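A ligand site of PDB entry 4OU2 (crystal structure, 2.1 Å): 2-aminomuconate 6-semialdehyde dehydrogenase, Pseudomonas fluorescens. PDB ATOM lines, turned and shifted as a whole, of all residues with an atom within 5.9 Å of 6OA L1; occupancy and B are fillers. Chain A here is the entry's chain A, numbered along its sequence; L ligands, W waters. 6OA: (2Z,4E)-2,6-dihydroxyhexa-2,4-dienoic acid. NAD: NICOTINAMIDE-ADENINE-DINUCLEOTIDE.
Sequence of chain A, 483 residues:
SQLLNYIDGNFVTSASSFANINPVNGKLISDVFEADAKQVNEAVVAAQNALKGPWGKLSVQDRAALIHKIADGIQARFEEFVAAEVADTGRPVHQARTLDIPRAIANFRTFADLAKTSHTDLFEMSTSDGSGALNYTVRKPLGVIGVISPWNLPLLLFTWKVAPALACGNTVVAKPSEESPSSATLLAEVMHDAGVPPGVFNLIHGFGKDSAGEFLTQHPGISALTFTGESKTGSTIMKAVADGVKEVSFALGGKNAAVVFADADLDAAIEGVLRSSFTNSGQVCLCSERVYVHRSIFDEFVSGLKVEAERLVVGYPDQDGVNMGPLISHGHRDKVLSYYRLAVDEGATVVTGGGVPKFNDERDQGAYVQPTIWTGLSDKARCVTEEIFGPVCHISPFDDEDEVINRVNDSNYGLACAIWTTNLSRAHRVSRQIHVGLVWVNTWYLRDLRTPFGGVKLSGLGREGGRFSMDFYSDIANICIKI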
ATOM      1  N   ARG A 103      20.681   5.806 -34.380  1.00  0.00           N
ATOM      2  CA  ARG A 103      21.397   6.459 -33.280  1.00  0.00           C
ATOM      3  C   ARG A 103      22.015   5.479 -32.320  1.00  0.00           C
ATOM      4  O   ARG A 103      23.145   5.691 -31.872  1.00  0.00           O
ATOM      5  CB  ARG A 103      20.517   7.404 -32.453  1.00  0.00           C
ATOM      6  CG  ARG A 103      20.637   8.855 -32.803  1.00  0.00           C
ATOM      7  CD  ARG A 103      22.026   9.455 -32.488  1.00  0.00           C
ATOM      8  NE  ARG A 103      22.412   9.324 -31.065  1.00  0.00           N
ATOM      9  CZ  ARG A 103      21.931  10.065 -30.075  1.00  0.00           C
ATOM     10  NH1 ARG A 103      20.972  11.015 -30.288  1.00  0.00           N
ATOM     11  NH2 ARG A 103      22.439   9.881 -28.848  1.00  0.00           N
ATOM     12  N   ASN A 107      25.815   5.598 -31.597  1.00  0.00           N
ATOM     13  CA  ASN A 107      26.331   5.720 -30.259  1.00  0.00           C
ATOM     14  C   ASN A 107      27.531   4.791 -30.088  1.00  0.00           C
ATOM     15  O   ASN A 107      28.555   5.214 -29.670  1.00  0.00           O
ATOM     16  CB  ASN A 107      25.260   5.390 -29.174  1.00  0.00           C
ATOM     17  CG  ASN A 107      24.218   6.487 -29.067  1.00  0.00           C
ATOM     18  OD1 ASN A 107      24.461   7.628 -29.471  1.00  0.00           O
ATOM     19  ND2 ASN A 107      23.066   6.165 -28.548  1.00  0.00           N
ATOM     20  N   ASN A 152      11.104   6.525 -23.102  1.00  0.00           N
ATOM     21  CA  ASN A 152      10.697   7.420 -24.193  1.00  0.00           C
ATOM     22  C   ASN A 152      11.514   7.258 -25.473  1.00  0.00           C
ATOM     23  O   ASN A 152      10.965   7.430 -26.599  1.00  0.00           O
ATOM     24  CB  ASN A 152      10.664   8.869 -23.703  1.00  0.00           C
ATOM     25  CG  ASN A 152      12.049   9.422 -23.449  1.00  0.00           C
ATOM     26  OD1 ASN A 152      12.916   8.743 -22.875  1.00  0.00           O
ATOM     27  ND2 ASN A 152      12.298  10.639 -23.940  1.00  0.00           N
ATOM     28  N   LEU A 153      12.813   6.964 -25.320  1.00  0.00           N
ATOM     29  CA  LEU A 153      13.712   6.636 -26.451  1.00  0.00           C
ATOM     30  C   LEU A 153      14.593   5.435 -26.045  1.00  0.00           C
ATOM     31  O   LEU A 153      15.782   5.590 -25.712  1.00  0.00           O
ATOM     32  CB  LEU A 153      14.614   7.829 -26.791  1.00  0.00           C
ATOM     33  CG  LEU A 153      13.876   9.125 -27.189  1.00  0.00           C
ATOM     34  CD1 LEU A 153      14.840  10.288 -27.174  1.00  0.00           C
ATOM     35  CD2 LEU A 153      13.248   8.932 -28.571  1.00  0.00           C
ATOM     36  N   LEU A 156      18.056   4.133 -27.909  1.00  0.00           N
ATOM     37  CA  LEU A 156      18.936   5.298 -28.092  1.00  0.00           C
ATOM     38  C   LEU A 156      19.517   5.728 -26.716  1.00  0.00           C
ATOM     39  O   LEU A 156      20.696   5.930 -26.595  1.00  0.00           O
ATOM     40  CB  LEU A 156      18.137   6.470 -28.714  1.00  0.00           C
ATOM     41  CG  LEU A 156      18.768   7.855 -29.065  1.00  0.00           C
ATOM     42  CD1 LEU A 156      17.921   8.565 -30.158  1.00  0.00           C
ATOM     43  CD2 LEU A 156      19.027   8.932 -27.920  1.00  0.00           C
ATOM     44  N   LEU A 157      18.669   5.812 -25.690  1.00  0.00           N
ATOM     45  CA  LEU A 157      19.123   6.314 -24.404  1.00  0.00           C
ATOM     46  C   LEU A 157      19.859   5.257 -23.639  1.00  0.00           C
ATOM     47  O   LEU A 157      20.765   5.581 -22.876  1.00  0.00           O
ATOM     48  CB  LEU A 157      17.974   6.859 -23.616  1.00  0.00           C
ATOM     49  CG  LEU A 157      17.506   8.257 -24.204  1.00  0.00           C
ATOM     50  CD1 LEU A 157      16.178   8.682 -23.541  1.00  0.00           C
ATOM     51  CD2 LEU A 157      18.589   9.296 -23.949  1.00  0.00           C
ATOM     52  N   TRP A 160      23.186   5.133 -25.352  1.00  0.00           N
ATOM     53  CA  TRP A 160      23.856   6.394 -25.083  1.00  0.00           C
ATOM     54  C   TRP A 160      24.748   6.296 -23.882  1.00  0.00           C
ATOM     55  O   TRP A 160      25.800   6.954 -23.783  1.00  0.00           O
ATOM     56  CB  TRP A 160      22.800   7.531 -24.935  1.00  0.00           C
ATOM     57  CG  TRP A 160      23.350   8.875 -24.559  1.00  0.00           C
ATOM     58  CD1 TRP A 160      23.086   9.602 -23.401  1.00  0.00           C
ATOM     59  CD2 TRP A 160      24.275   9.702 -25.327  1.00  0.00           C
ATOM     60  NE1 TRP A 160      23.802  10.786 -23.410  1.00  0.00           N
ATOM     61  CE2 TRP A 160      24.527  10.892 -24.544  1.00  0.00           C
ATOM     62  CE3 TRP A 160      24.925   9.556 -26.566  1.00  0.00           C
ATOM     63  CZ2 TRP A 160      25.364  11.910 -24.999  1.00  0.00           C
ATOM     64  CZ3 TRP A 160      25.800  10.600 -27.005  1.00  0.00           C
ATOM     65  CH2 TRP A 160      26.013  11.727 -26.236  1.00  0.00           C
ATOM     66  N   THR A 228      18.962   8.512 -16.677  1.00  0.00           N
ATOM     67  CA  THR A 228      18.103   9.436 -17.417  1.00  0.00           C
ATOM     68  C   THR A 228      16.630   9.164 -17.030  1.00  0.00           C
ATOM     69  O   THR A 228      16.188   8.019 -16.953  1.00  0.00           O
ATOM     70  CB  THR A 228      18.313   9.251 -18.917  1.00  0.00           C
ATOM     71  OG1 THR A 228      19.643   9.628 -19.300  1.00  0.00           O
ATOM     72  CG2 THR A 228      17.405  10.160 -19.667  1.00  0.00           C
ATOM     73  N   GLN A 283       6.602  13.119 -26.087  1.00  0.00           N
ATOM     74  CA  GLN A 283       7.299  12.333 -25.050  1.00  0.00           C
ATOM     75  C   GLN A 283       8.802  12.364 -25.277  1.00  0.00           C
ATOM     76  O   GLN A 283       9.458  11.337 -25.156  1.00  0.00           O
ATOM     77  CB  GLN A 283       6.810  10.900 -25.033  1.00  0.00           C
ATOM     78  CG  GLN A 283       5.319  10.755 -24.784  1.00  0.00           C
ATOM     79  CD  GLN A 283       4.839   9.323 -24.972  1.00  0.00           C
ATOM     80  OE1 GLN A 283       4.259   8.727 -24.068  1.00  0.00           O
ATOM     81  NE2 GLN A 283       5.082   8.760 -26.147  1.00  0.00           N
ATOM     82  N   VAL A 284       9.339  13.544 -25.581  1.00  0.00           N
ATOM     83  CA  VAL A 284      10.797  13.755 -25.583  1.00  0.00           C
ATOM     84  C   VAL A 284      11.120  14.785 -24.474  1.00  0.00           C
ATOM     85  O   VAL A 284      10.382  15.738 -24.252  1.00  0.00           O
ATOM     86  CB  VAL A 284      11.330  14.245 -26.925  1.00  0.00           C
ATOM     87  CG1 VAL A 284      12.835  14.086 -26.961  1.00  0.00           C
ATOM     88  CG2 VAL A 284      10.697  13.477 -28.078  1.00  0.00           C
ATOM     89  N   CYS A 285      12.238  14.596 -23.781  1.00  0.00           N
ATOM     90  CA  CYS A 285      12.543  15.450 -22.654  1.00  0.00           C
ATOM     91  C   CYS A 285      12.850  16.846 -23.151  1.00  0.00           C
ATOM     92  O   CYS A 285      12.621  17.846 -22.440  1.00  0.00           O
ATOM     93  CB  CYS A 285      13.745  14.896 -21.884  1.00  0.00           C
ATOM     94  SG  CYS A 285      15.257  14.886 -22.905  1.00  0.00           S
ATOM     95  N   LEU A 286      13.334  16.916 -24.377  1.00  0.00           N
ATOM     96  CA  LEU A 286      13.626  18.174 -25.057  1.00  0.00           C
ATOM     97  C   LEU A 286      12.420  18.943 -25.640  1.00  0.00           C
ATOM     98  O   LEU A 286      12.592  20.047 -26.184  1.00  0.00           O
ATOM     99  CB  LEU A 286      14.629  17.914 -26.195  1.00  0.00           C
ATOM    100  CG  LEU A 286      15.838  17.101 -25.722  1.00  0.00           C
ATOM    101  CD1 LEU A 286      16.516  16.594 -26.981  1.00  0.00           C
ATOM    102  CD2 LEU A 286      16.763  18.029 -24.924  1.00  0.00           C
ATOM    103  N   PHE A 389       4.896  15.966 -20.277  1.00  0.00           N
ATOM    104  CA  PHE A 389       5.453  14.858 -21.026  1.00  0.00           C
ATOM    105  C   PHE A 389       4.407  14.225 -21.944  1.00  0.00           C
ATOM    106  O   PHE A 389       4.276  13.017 -22.067  1.00  0.00           O
ATOM    107  CB  PHE A 389       6.124  13.768 -20.074  1.00  0.00           C
ATOM    108  CG  PHE A 389       7.380  13.190 -20.666  1.00  0.00           C
ATOM    109  CD1 PHE A 389       7.425  11.856 -21.053  1.00  0.00           C
ATOM    110  CD2 PHE A 389       8.480  13.993 -20.909  1.00  0.00           C
ATOM    111  CE1 PHE A 389       8.584  11.330 -21.639  1.00  0.00           C
ATOM    112  CE2 PHE A 389       9.632  13.472 -21.501  1.00  0.00           C
ATOM    113  CZ  PHE A 389       9.673  12.144 -21.876  1.00  0.00           C
ATOM    114  N   LEU A 415      16.674  22.442 -19.111  1.00  0.00           N
ATOM    115  CA  LEU A 415      17.229  21.429 -19.992  1.00  0.00           C
ATOM    116  C   LEU A 415      17.554  22.026 -21.321  1.00  0.00           C
ATOM    117  O   LEU A 415      18.749  22.096 -21.728  1.00  0.00           O
ATOM    118  CB  LEU A 415      16.267  20.236 -20.100  1.00  0.00           C
ATOM    119  CG  LEU A 415      16.731  19.136 -21.010  1.00  0.00           C
ATOM    120  CD1 LEU A 415      18.197  18.687 -20.652  1.00  0.00           C
ATOM    121  CD2 LEU A 415      15.758  17.948 -20.940  1.00  0.00           C
ATOM    122  N   TYR A 445      16.341  19.726 -31.576  1.00  0.00           N
ATOM    123  CA  TYR A 445      16.885  18.340 -31.426  1.00  0.00           C
ATOM    124  C   TYR A 445      17.756  17.952 -32.603  1.00  0.00           C
ATOM    125  O   TYR A 445      17.599  16.888 -33.126  1.00  0.00           O
ATOM    126  CB  TYR A 445      15.755  17.299 -31.254  1.00  0.00           C
ATOM    127  CG  TYR A 445      16.210  15.926 -30.700  1.00  0.00           C
ATOM    128  CD1 TYR A 445      17.422  15.788 -29.999  1.00  0.00           C
ATOM    129  CD2 TYR A 445      15.479  14.781 -30.866  1.00  0.00           C
ATOM    130  CE1 TYR A 445      17.903  14.571 -29.475  1.00  0.00           C
ATOM    131  CE2 TYR A 445      15.969  13.529 -30.329  1.00  0.00           C
ATOM    132  CZ  TYR A 445      17.234  13.400 -29.631  1.00  0.00           C
ATOM    133  OH  TYR A 445      17.836  12.227 -29.045  1.00  0.00           O
ATOM    134  N   ARG A 447      21.408  16.877 -33.309  1.00  0.00           N
ATOM    135  CA  ARG A 447      22.452  16.373 -32.378  1.00  0.00           C
ATOM    136  C   ARG A 447      23.762  16.046 -33.072  1.00  0.00           C
ATOM    137  O   ARG A 447      23.790  15.331 -34.044  1.00  0.00           O
ATOM    138  CB  ARG A 447      22.003  15.135 -31.587  1.00  0.00           C
ATOM    139  CG  ARG A 447      20.822  15.406 -30.652  1.00  0.00           C
ATOM    140  CD  ARG A 447      21.235  15.749 -29.222  1.00  0.00           C
ATOM    141  NE  ARG A 447      22.046  14.669 -28.619  1.00  0.00           N
ATOM    142  CZ  ARG A 447      23.316  14.812 -28.210  1.00  0.00           C
ATOM    143  NH1 ARG A 447      23.915  16.004 -28.290  1.00  0.00           N
ATOM    144  NH2 ARG A 447      23.971  13.773 -27.691  1.00  0.00           N
ATOM    145  N   LEU A 449      27.059  14.282 -31.786  1.00  0.00           N
ATOM    146  CA  LEU A 449      27.340  13.430 -30.678  1.00  0.00           C
ATOM    147  C   LEU A 449      28.570  13.830 -29.874  1.00  0.00           C
ATOM    148  O   LEU A 449      28.826  13.266 -28.807  1.00  0.00           O
ATOM    149  CB  LEU A 449      27.347  11.959 -31.100  1.00  0.00           C
ATOM    150  CG  LEU A 449      25.999  11.437 -31.682  1.00  0.00           C
ATOM    151  CD1 LEU A 449      26.107   9.894 -31.939  1.00  0.00           C
ATOM    152  CD2 LEU A 449      24.864  11.692 -30.705  1.00  0.00           C
ATOM    153  N   PHE A 453      26.150  17.412 -23.379  1.00  0.00           N
ATOM    154  CA  PHE A 453      24.713  17.281 -23.302  1.00  0.00           C
ATOM    155  C   PHE A 453      24.291  17.128 -21.853  1.00  0.00           C
ATOM    156  O   PHE A 453      24.816  16.244 -21.101  1.00  0.00           O
ATOM    157  CB  PHE A 453      24.244  16.069 -24.135  1.00  0.00           C
ATOM    158  CG  PHE A 453      22.766  15.867 -24.077  1.00  0.00           C
ATOM    159  CD1 PHE A 453      22.128  15.388 -22.937  1.00  0.00           C
ATOM    160  CD2 PHE A 453      21.992  16.179 -25.213  1.00  0.00           C
ATOM    161  CE1 PHE A 453      20.734  15.255 -22.919  1.00  0.00           C
ATOM    162  CE2 PHE A 453      20.627  16.025 -25.216  1.00  0.00           C
ATOM    163  CZ  PHE A 453      19.992  15.561 -24.082  1.00  0.00           C
HETATM  164  O3  6OA L   1      14.048  12.518 -24.002  1.00  0.00           O
HETATM  165  C5  6OA L   1      15.295  13.251 -23.790  1.00  0.00           C
HETATM  166  C4  6OA L   1      16.200  13.109 -24.990  1.00  0.00           C
HETATM  167  C3  6OA L   1      17.504  12.862 -24.776  1.00  0.00           C
HETATM  168  C2  6OA L   1      18.358  12.696 -25.991  1.00  0.00           C
HETATM  169  C1  6OA L   1      19.648  12.459 -25.846  1.00  0.00           C
HETATM  170  O2  6OA L   1      20.150  12.310 -24.614  1.00  0.00           O
HETATM  171  C   6OA L   1      20.514  12.313 -26.999  1.00  0.00           C
HETATM  172  O1  6OA L   1      21.640  11.878 -26.901  1.00  0.00           O
HETATM  173  O   6OA L   1      20.072  12.665 -28.197  1.00  0.00           O
HETATM  174  PA  NAD L   2      11.114   7.319 -14.422  1.00  0.00           P
HETATM  175  O1A NAD L   2      12.027   8.369 -13.657  1.00  0.00           O
HETATM  176  O2A NAD L   2      10.257   7.498 -13.149  1.00  0.00           O
HETATM  177  O5B NAD L   2      12.269   6.206 -14.363  1.00  0.00           O
HETATM  178  C5B NAD L   2      12.982   5.799 -15.487  1.00  0.00           C
HETATM  179  C4B NAD L   2      13.834   4.627 -15.071  1.00  0.00           C
HETATM  180  O4B NAD L   2      14.220   4.717 -13.713  1.00  0.00           O
HETATM  181  C3B NAD L   2      13.124   3.311 -15.209  1.00  0.00           C
HETATM  182  O3B NAD L   2      14.045   2.367 -15.621  1.00  0.00           O
HETATM  183  C2B NAD L   2      12.610   3.018 -13.862  1.00  0.00           C
HETATM  184  O2B NAD L   2      12.406   1.659 -13.598  1.00  0.00           O
HETATM  185  C1B NAD L   2      13.744   3.589 -13.047  1.00  0.00           C
HETATM  186  N9A NAD L   2      13.415   3.935 -11.690  1.00  0.00           N
HETATM  187  C8A NAD L   2      12.288   4.566 -11.272  1.00  0.00           C
HETATM  188  N7A NAD L   2      12.321   4.727  -9.942  1.00  0.00           N
HETATM  189  C5A NAD L   2      13.467   4.227  -9.470  1.00  0.00           C
HETATM  190  C6A NAD L   2      14.039   4.129  -8.198  1.00  0.00           C
HETATM  191  N6A NAD L   2      13.307   4.626  -7.054  1.00  0.00           N
HETATM  192  N1A NAD L   2      15.262   3.583  -8.051  1.00  0.00           N
HETATM  193  C2A NAD L   2      15.954   3.090  -9.120  1.00  0.00           C
HETATM  194  N3A NAD L   2      15.428   3.135 -10.389  1.00  0.00           N
HETATM  195  C4A NAD L   2      14.207   3.688 -10.590  1.00  0.00           C
HETATM  196  O3  NAD L   2      11.224   8.377 -15.615  1.00  0.00           O
HETATM  197  PN  NAD L   2      10.415   8.100 -17.001  1.00  0.00           P
HETATM  198  O1N NAD L   2       8.914   8.166 -16.715  1.00  0.00           O
HETATM  199  O2N NAD L   2      10.815   6.710 -17.484  1.00  0.00           O
HETATM  200  O5D NAD L   2      10.789   9.157 -18.133  1.00  0.00           O
HETATM  201  C5D NAD L   2      10.096  10.357 -18.240  1.00  0.00           C
HETATM  202  C4D NAD L   2      10.971  11.358 -17.555  1.00  0.00           C
HETATM  203  O4D NAD L   2      12.321  11.143 -17.934  1.00  0.00           O
HETATM  204  C3D NAD L   2      10.642  12.786 -17.868  1.00  0.00           C
HETATM  205  O3D NAD L   2      10.849  13.603 -16.748  1.00  0.00           O
HETATM  206  C2D NAD L   2      11.651  13.030 -18.939  1.00  0.00           C
HETATM  207  O2D NAD L   2      11.865  14.347 -19.378  1.00  0.00           O
HETATM  208  C1D NAD L   2      12.842  12.375 -18.337  1.00  0.00           C
HETATM  209  N1N NAD L   2      13.792  12.204 -19.373  1.00  0.00           N
HETATM  210  C2N NAD L   2      14.868  13.053 -19.382  1.00  0.00           C
HETATM  211  C3N NAD L   2      15.797  12.942 -20.406  1.00  0.00           C
HETATM  212  C7N NAD L   2      17.025  13.881 -20.482  1.00  0.00           C
HETATM  213  O7N NAD L   2      18.006  13.676 -21.281  1.00  0.00           O
HETATM  214  N7N NAD L   2      17.053  15.018 -19.634  1.00  0.00           N
HETATM  215  C4N NAD L   2      15.611  11.896 -21.341  1.00  0.00           C
HETATM  216  C5N NAD L   2      14.554  11.000 -21.327  1.00  0.00           C
HETATM  217  C6N NAD L   2      13.627  11.179 -20.295  1.00  0.00           C
HETATM  218  O   HOH W   1      20.134  11.679 -21.623  1.00  0.00           O
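An oxygen (O3) of 6OA L1 is in hydrogen-bond range of the backbone NH (N) of Cys 285 (2.8 Å).
SG of Cys 285 is bonded to C5 of 6OA L1.
An oxygen (O) of 6OA L1 is in hydrogen-bond range of the side-chain hydroxyl (OH) of Tyr 445 (2.4 Å).
An oxygen (O3) of 6OA L1 lies within hydrogen-bond range of the side-chain amide nitrogen of Asn 152, at 2.6 Å.
The guanidinium group of Arg 103 lies within salt-bridge range of an oxygen (O) of 6OA L1, 2.8 Å away.
The guanidinium group (NE) of Arg 447 lies within salt-bridge range of an oxygen (O) of 6OA L1 (2.8 Å).
SG of Cys 285 sits close to N7N of NAD L2 (3.7 Å).
O of Gln 283 sits close to ND2 of Asn 152 (3.2 Å).
NH2 of Arg 103 is in hydrogen-bond range of OD1 of Asn 107.
N of Trp 160 sits close to ND2 of Asn 107 (3.4 Å).
The side-chain amide nitrogen (ND2) of Asn 107 is in hydrogen-bond range of the backbone carbonyl oxygen (O) of Leu 156, 3.1 Å away.
Merely in contact with 6OA L1: Phe 453 (3.3 Å), Leu 157 (3.5 Å), Val 284 (3.6 Å), Trp 160 (3.8 Å), Leu 156 (3.8 Å) and Leu 153 (3.8 Å).
Hydrophobic or aromatic side chains that line 6OA L1: Leu 153, Leu 156, Leu 157, Trp 160, Val 284, Tyr 445 and Phe 453.
Of the 18 residues printed, 11 come within 4 Å of 6OA L1.
The nearest printed residue that does not touch 6OA L1 is Leu 286 (4.03 Å).
Water W1 lies within hydrogen-bond range of an oxygen (O7N) of NAD L2, an oxygen (O2) of 6OA L1 and the side-chain hydroxyl (OG1) of Thr 228.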
